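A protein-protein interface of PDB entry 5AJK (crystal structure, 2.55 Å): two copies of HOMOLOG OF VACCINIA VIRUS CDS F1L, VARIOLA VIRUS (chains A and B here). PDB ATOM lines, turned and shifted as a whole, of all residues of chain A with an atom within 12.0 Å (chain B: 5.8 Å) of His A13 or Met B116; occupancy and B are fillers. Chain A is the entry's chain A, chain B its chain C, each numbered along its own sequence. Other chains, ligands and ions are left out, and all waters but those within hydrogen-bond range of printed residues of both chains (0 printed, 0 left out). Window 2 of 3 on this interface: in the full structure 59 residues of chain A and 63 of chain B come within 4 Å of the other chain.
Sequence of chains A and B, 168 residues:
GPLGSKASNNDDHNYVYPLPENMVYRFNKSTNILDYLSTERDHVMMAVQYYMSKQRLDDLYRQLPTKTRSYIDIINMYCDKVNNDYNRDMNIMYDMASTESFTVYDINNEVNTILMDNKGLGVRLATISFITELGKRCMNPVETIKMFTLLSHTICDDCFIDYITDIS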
ATOM      1  N   HIS A  13     -25.538   7.263   0.442  1.00  0.00           N
ATOM      2  CA  HIS A  13     -25.953   7.907   1.684  1.00  0.00           C
ATOM      3  C   HIS A  13     -26.825   9.129   1.403  1.00  0.00           C
ATOM      4  O   HIS A  13     -26.606  10.205   1.962  1.00  0.00           O
ATOM      5  CB  HIS A  13     -24.728   8.302   2.518  1.00  0.00           C
ATOM      6  CG  HIS A  13     -24.109   7.155   3.258  1.00  0.00           C
ATOM      7  ND1 HIS A  13     -24.706   6.575   4.352  1.00  0.00           N
ATOM      8  CD2 HIS A  13     -22.950   6.482   3.053  1.00  0.00           C
ATOM      9  CE1 HIS A  13     -23.942   5.588   4.795  1.00  0.00           C
ATOM     10  NE2 HIS A  13     -22.875   5.513   4.027  1.00  0.00           N
ATOM     11  N   ASN A  14     -27.820   8.959   0.538  1.00  0.00           N
ATOM     12  CA  ASN A  14     -28.764  10.034   0.250  1.00  0.00           C
ATOM     13  C   ASN A  14     -29.755  10.146   1.411  1.00  0.00           C
ATOM     14  O   ASN A  14     -29.482   9.672   2.513  1.00  0.00           O
ATOM     15  CB  ASN A  14     -29.488   9.783  -1.085  1.00  0.00           C
ATOM     16  CG  ASN A  14     -29.636  11.048  -1.931  1.00  0.00           C
ATOM     17  OD1 ASN A  14     -29.253  12.142  -1.518  1.00  0.00           O
ATOM     18  ND2 ASN A  14     -30.182  10.890  -3.133  1.00  0.00           N
ATOM     19  N   TYR A  15     -30.899  10.776   1.170  1.00  0.00           N
ATOM     20  CA  TYR A  15     -31.917  10.910   2.203  1.00  0.00           C
ATOM     21  C   TYR A  15     -32.439   9.547   2.635  1.00  0.00           C
ATOM     22  O   TYR A  15     -32.193   8.539   1.975  1.00  0.00           O
ATOM     23  CB  TYR A  15     -33.073  11.778   1.709  1.00  0.00           C
ATOM     24  CG  TYR A  15     -32.653  13.163   1.267  1.00  0.00           C
ATOM     25  CD1 TYR A  15     -32.291  14.130   2.196  1.00  0.00           C
ATOM     26  CD2 TYR A  15     -32.622  13.505  -0.079  1.00  0.00           C
ATOM     27  CE1 TYR A  15     -31.906  15.395   1.796  1.00  0.00           C
ATOM     28  CE2 TYR A  15     -32.240  14.770  -0.487  1.00  0.00           C
ATOM     29  CZ  TYR A  15     -31.884  15.711   0.456  1.00  0.00           C
ATOM     30  OH  TYR A  15     -31.503  16.971   0.055  1.00  0.00           O
ATOM     31  N   VAL A  16     -33.160   9.531   3.751  1.00  0.00           N
ATOM     32  CA  VAL A  16     -33.706   8.301   4.304  1.00  0.00           C
ATOM     33  C   VAL A  16     -35.221   8.396   4.368  1.00  0.00           C
ATOM     34  O   VAL A  16     -35.771   9.364   4.889  1.00  0.00           O
ATOM     35  CB  VAL A  16     -33.148   8.019   5.706  1.00  0.00           C
ATOM     36  CG1 VAL A  16     -33.735   6.737   6.257  1.00  0.00           C
ATOM     37  CG2 VAL A  16     -31.632   7.927   5.656  1.00  0.00           C
ATOM     38  N   TYR A  17     -35.892   7.387   3.829  1.00  0.00           N
ATOM     39  CA  TYR A  17     -37.343   7.350   3.863  1.00  0.00           C
ATOM     40  C   TYR A  17     -37.783   7.065   5.298  1.00  0.00           C
ATOM     41  O   TYR A  17     -37.338   6.082   5.891  1.00  0.00           O
ATOM     42  CB  TYR A  17     -37.874   6.288   2.899  1.00  0.00           C
ATOM     43  CG  TYR A  17     -39.283   6.545   2.411  1.00  0.00           C
ATOM     44  CD1 TYR A  17     -39.525   7.393   1.338  1.00  0.00           C
ATOM     45  CD2 TYR A  17     -40.369   5.936   3.022  1.00  0.00           C
ATOM     46  CE1 TYR A  17     -40.813   7.628   0.887  1.00  0.00           C
ATOM     47  CE2 TYR A  17     -41.657   6.166   2.582  1.00  0.00           C
ATOM     48  CZ  TYR A  17     -41.874   7.011   1.515  1.00  0.00           C
ATOM     49  OH  TYR A  17     -43.160   7.235   1.080  1.00  0.00           O
ATOM     50  N   ARG A  41     -25.128  -7.825   2.354  1.00  0.00           N
ATOM     51  CA  ARG A  41     -25.641  -6.697   3.116  1.00  0.00           C
ATOM     52  C   ARG A  41     -26.650  -7.184   4.145  1.00  0.00           C
ATOM     53  O   ARG A  41     -26.655  -6.725   5.288  1.00  0.00           O
ATOM     54  CB  ARG A  41     -26.285  -5.659   2.194  1.00  0.00           C
ATOM     55  CG  ARG A  41     -26.905  -4.485   2.932  1.00  0.00           C
ATOM     56  CD  ARG A  41     -27.238  -3.333   2.004  1.00  0.00           C
ATOM     57  NE  ARG A  41     -27.583  -2.126   2.754  1.00  0.00           N
ATOM     58  CZ  ARG A  41     -28.806  -1.820   3.184  1.00  0.00           C
ATOM     59  NH1 ARG A  41     -29.834  -2.625   2.940  1.00  0.00           N
ATOM     60  NH2 ARG A  41     -29.003  -0.698   3.862  1.00  0.00           N
ATOM     61  N   MET A  45     -26.086  -6.795   8.126  1.00  0.00           N
ATOM     62  CA  MET A  45     -27.119  -6.037   8.824  1.00  0.00           C
ATOM     63  C   MET A  45     -27.739  -6.878   9.925  1.00  0.00           C
ATOM     64  O   MET A  45     -28.015  -6.381  11.016  1.00  0.00           O
ATOM     65  CB  MET A  45     -28.210  -5.570   7.862  1.00  0.00           C
ATOM     66  CG  MET A  45     -27.929  -4.240   7.199  1.00  0.00           C
ATOM     67  SD  MET A  45     -29.425  -3.490   6.530  1.00  0.00           S
ATOM     68  CE  MET A  45     -30.007  -4.792   5.445  1.00  0.00           C
ATOM     69  N   VAL B 111     -25.199  10.531  11.401  1.00  0.00           N
ATOM     70  CA  VAL B 111     -24.366   9.392  11.040  1.00  0.00           C
ATOM     71  C   VAL B 111     -24.333   9.230   9.526  1.00  0.00           C
ATOM     72  O   VAL B 111     -23.278   8.976   8.947  1.00  0.00           O
ATOM     73  CB  VAL B 111     -24.875   8.088  11.691  1.00  0.00           C
ATOM     74  CG1 VAL B 111     -24.127   6.870  11.140  1.00  0.00           C
ATOM     75  CG2 VAL B 111     -24.733   8.157  13.206  1.00  0.00           C
ATOM     76  N   ASN B 112     -25.493   9.386   8.893  1.00  0.00           N
ATOM     77  CA  ASN B 112     -25.603   9.268   7.443  1.00  0.00           C
ATOM     78  C   ASN B 112     -24.691  10.275   6.748  1.00  0.00           C
ATOM     79  O   ASN B 112     -23.984   9.936   5.799  1.00  0.00           O
ATOM     80  CB  ASN B 112     -27.055   9.472   6.997  1.00  0.00           C
ATOM     81  CG  ASN B 112     -27.326   8.929   5.603  1.00  0.00           C
ATOM     82  OD1 ASN B 112     -26.869   7.843   5.246  1.00  0.00           O
ATOM     83  ND2 ASN B 112     -28.076   9.684   4.810  1.00  0.00           N
ATOM     84  N   THR B 113     -24.702  11.510   7.242  1.00  0.00           N
ATOM     85  CA  THR B 113     -23.886  12.580   6.675  1.00  0.00           C
ATOM     86  C   THR B 113     -22.393  12.289   6.809  1.00  0.00           C
ATOM     87  O   THR B 113     -21.626  12.507   5.872  1.00  0.00           O
ATOM     88  CB  THR B 113     -24.184  13.933   7.355  1.00  0.00           C
ATOM     89  OG1 THR B 113     -25.584  14.224   7.261  1.00  0.00           O
ATOM     90  CG2 THR B 113     -23.393  15.059   6.700  1.00  0.00           C
ATOM     91  N   ILE B 114     -21.986  11.809   7.979  1.00  0.00           N
ATOM     92  CA  ILE B 114     -20.574  11.577   8.259  1.00  0.00           C
ATOM     93  C   ILE B 114     -20.042  10.348   7.516  1.00  0.00           C
ATOM     94  O   ILE B 114     -18.888  10.330   7.088  1.00  0.00           O
ATOM     95  CB  ILE B 114     -20.337  11.431   9.789  1.00  0.00           C
ATOM     96  CG1 ILE B 114     -19.894  12.764  10.395  1.00  0.00           C
ATOM     97  CG2 ILE B 114     -19.275  10.384  10.117  1.00  0.00           C
ATOM     98  CD1 ILE B 114     -21.007  13.537  11.048  1.00  0.00           C
ATOM     99  N   LEU B 115     -20.879   9.331   7.344  1.00  0.00           N
ATOM    100  CA  LEU B 115     -20.450   8.126   6.642  1.00  0.00           C
ATOM    101  C   LEU B 115     -20.402   8.344   5.129  1.00  0.00           C
ATOM    102  O   LEU B 115     -19.736   7.600   4.410  1.00  0.00           O
ATOM    103  CB  LEU B 115     -21.375   6.951   6.968  1.00  0.00           C
ATOM    104  CG  LEU B 115     -21.292   6.314   8.359  1.00  0.00           C
ATOM    105  CD1 LEU B 115     -21.894   4.918   8.293  1.00  0.00           C
ATOM    106  CD2 LEU B 115     -19.869   6.258   8.897  1.00  0.00           C
ATOM    107  N   MET B 116     -21.103   9.364   4.646  1.00  0.00           N
ATOM    108  CA  MET B 116     -21.128   9.659   3.217  1.00  0.00           C
ATOM    109  C   MET B 116     -19.767  10.145   2.733  1.00  0.00           C
ATOM    110  O   MET B 116     -19.338   9.824   1.625  1.00  0.00           O
ATOM    111  CB  MET B 116     -22.194  10.708   2.909  1.00  0.00           C
ATOM    112  CG  MET B 116     -22.233  11.160   1.461  1.00  0.00           C
ATOM    113  SD  MET B 116     -23.504  12.405   1.206  1.00  0.00           S
ATOM    114  CE  MET B 116     -22.667  13.495   0.058  1.00  0.00           C
ATOM    115  N   ASP B 117     -19.100  10.930   3.572  1.00  0.00           N
ATOM    116  CA  ASP B 117     -17.808  11.514   3.231  1.00  0.00           C
ATOM    117  C   ASP B 117     -16.661  10.657   3.763  1.00  0.00           C
ATOM    118  O   ASP B 117     -15.607  10.552   3.136  1.00  0.00           O
ATOM    119  CB  ASP B 117     -17.710  12.936   3.789  1.00  0.00           C
ATOM    120  CG  ASP B 117     -18.871  13.815   3.354  1.00  0.00           C
ATOM    121  OD1 ASP B 117     -19.290  13.715   2.181  1.00  0.00           O
ATOM    122  OD2 ASP B 117     -19.367  14.603   4.186  1.00  0.00           O
ATOM    123  N   ASN B 118     -16.882  10.041   4.923  1.00  0.00           N
ATOM    124  CA  ASN B 118     -15.876   9.206   5.573  1.00  0.00           C
ATOM    125  C   ASN B 118     -16.108   7.732   5.233  1.00  0.00           C
ATOM    126  O   ASN B 118     -17.190   7.199   5.477  1.00  0.00           O
ATOM    127  CB  ASN B 118     -15.910   9.427   7.089  1.00  0.00           C
ATOM    128  CG  ASN B 118     -14.645   8.958   7.782  1.00  0.00           C
ATOM    129  OD1 ASN B 118     -14.093   7.910   7.450  1.00  0.00           O
ATOM    130  ND2 ASN B 118     -14.178   9.739   8.752  1.00  0.00           N
ATOM    131  N   LYS B 119     -15.091   7.084   4.667  1.00  0.00           N
ATOM    132  CA  LYS B 119     -15.223   5.719   4.151  1.00  0.00           C
ATOM    133  C   LYS B 119     -14.343   4.693   4.872  1.00  0.00           C
ATOM    134  O   LYS B 119     -14.175   3.570   4.394  1.00  0.00           O
ATOM    135  CB  LYS B 119     -14.899   5.706   2.653  1.00  0.00           C
ATOM    136  CG  LYS B 119     -15.896   6.478   1.797  1.00  0.00           C
ATOM    137  CD  LYS B 119     -17.270   5.819   1.805  1.00  0.00           C
ATOM    138  CE  LYS B 119     -18.301   6.660   1.079  1.00  0.00           C
ATOM    139  NZ  LYS B 119     -19.686   6.192   1.365  1.00  0.00           N
ATOM    140  N   ARG B 124     -17.243   3.462  11.373  1.00  0.00           N
ATOM    141  CA  ARG B 124     -18.381   2.552  11.368  1.00  0.00           C
ATOM    142  C   ARG B 124     -18.406   1.687  12.624  1.00  0.00           C
ATOM    143  O   ARG B 124     -19.459   1.506  13.232  1.00  0.00           O
ATOM    144  CB  ARG B 124     -18.355   1.682  10.110  1.00  0.00           C
ATOM    145  CG  ARG B 124     -18.937   2.386   8.898  1.00  0.00           C
ATOM    146  CD  ARG B 124     -18.191   2.050   7.622  1.00  0.00           C
ATOM    147  NE  ARG B 124     -18.695   2.841   6.501  1.00  0.00           N
ATOM    148  CZ  ARG B 124     -18.262   4.058   6.180  1.00  0.00           C
ATOM    149  NH1 ARG B 124     -17.295   4.641   6.883  1.00  0.00           N
ATOM    150  NH2 ARG B 124     -18.790   4.698   5.147  1.00  0.00           N
ATOM    151  N   THR B 154     -28.027   2.456   7.912  1.00  0.00           N
ATOM    152  CA  THR B 154     -27.092   3.519   7.566  1.00  0.00           C
ATOM    153  C   THR B 154     -25.646   3.045   7.652  1.00  0.00           C
ATOM    154  O   THR B 154     -24.840   3.327   6.770  1.00  0.00           O
ATOM    155  CB  THR B 154     -27.273   4.738   8.487  1.00  0.00           C
ATOM    156  OG1 THR B 154     -28.606   5.244   8.355  1.00  0.00           O
ATOM    157  CG2 THR B 154     -26.286   5.840   8.131  1.00  0.00           C
ATOM    158  N   ILE B 155     -25.319   2.324   8.717  1.00  0.00           N
ATOM    159  CA  ILE B 155     -23.949   1.869   8.935  1.00  0.00           C
ATOM    160  C   ILE B 155     -23.540   0.825   7.901  1.00  0.00           C
ATOM    161  O   ILE B 155     -22.447   0.890   7.340  1.00  0.00           O
ATOM    162  CB  ILE B 155     -23.774   1.281  10.350  1.00  0.00           C
ATOM    163  CG1 ILE B 155     -24.048   2.354  11.407  1.00  0.00           C
ATOM    164  CG2 ILE B 155     -22.363   0.729  10.539  1.00  0.00           C
ATOM    165  CD1 ILE B 155     -24.290   1.799  12.793  1.00  0.00           C
ATOM    166  N   ASP B 157     -23.388   0.188   4.923  1.00  0.00           N
ATOM    167  CA  ASP B 157     -23.271   0.609   3.534  1.00  0.00           C
ATOM    168  C   ASP B 157     -22.301  -0.322   2.809  1.00  0.00           C
ATOM    169  O   ASP B 157     -21.812  -1.290   3.392  1.00  0.00           O
ATOM    170  CB  ASP B 157     -22.819   2.070   3.443  1.00  0.00           C
ATOM    171  CG  ASP B 157     -21.485   2.320   4.121  1.00  0.00           C
ATOM    172  OD1 ASP B 157     -20.994   1.424   4.837  1.00  0.00           O
ATOM    173  OD2 ASP B 157     -20.933   3.426   3.943  1.00  0.00           O
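A ring nitrogen (NE2) of His A13 lies within hydrogen-bond range of the side-chain carboxylate of Asp B157 (2.9 Å).
O of Asn A14 is in hydrogen-bond range of ND2 of Asn B112, at 2.7 Å.
A ring nitrogen (ND1) of His A13 lies within hydrogen-bond range of the side-chain amide oxygen (OD1) of Asn B112, 2.7 Å away.
The guanidinium group (NH2) of Arg B124 lies within salt-bridge range of the side-chain carboxylate (OD2) of Asp B157.
The guanidinium group of Arg B124 lies within hydrogen-bond range of the backbone carbonyl oxygen of Leu B115.
NZ of Lys B119 sits at hydrogen-bond distance from O of Leu B115 (3.4 Å).
The side-chain amino group of Lys B119 is in salt-bridge range of the side-chain carboxylate of Asp B157, at 3.98 Å.
Among the printed residues, pairs that only touch across the chains: His A13 with Thr B154, His A13 with Met B116, His A13 with Leu B115 and His A13 with Lys B119.
Of chain B, only Asn B112 (2.7 Å), Leu B115 (3.6 Å), Met B116 (3.5 Å), Lys B119 (3.7 Å), Thr B154 (3.1 Å) and Asp B157 (2.9 Å) come within 4 Å of His A13.
Of chain A, only His A13 (3.5 Å) comes within 4 Å of Met B116.
Of the printed residues of chain A, Asn B112 touches His A13 and Asn A14.
Thr B113 touches none of the printed residues of chain A.
No residue of chain A comes within 4 Å of Ile B114.
Asp B157 touches just one residue of chain A: His A13 (2.9 Å).
Of the printed residues of chain A, Lys B119 touches His A13.
Of the printed residues of chain B, Asn A14 touches Asn B112 (2.7 Å).
The nearest residue of chain A that does not touch Met B116 is Asn A14 (5.6 Å).
The nearest printed residue of chain A that does not touch Lys B119 is Asn A14 (8.6 Å).
Of the 7 printed residues of chain A, 2 touch a printed residue of chain B.
Of the 13 printed residues of chain B, 6 touch a printed residue of chain A.
Along chain B the printed residues that touch a printed residue of chain A span positions 112 to 157.
No position is printed for both chains.
Of the 7 pairs that touch across the chains among the printed residues, none has its exchanged pair printed and touching as well.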
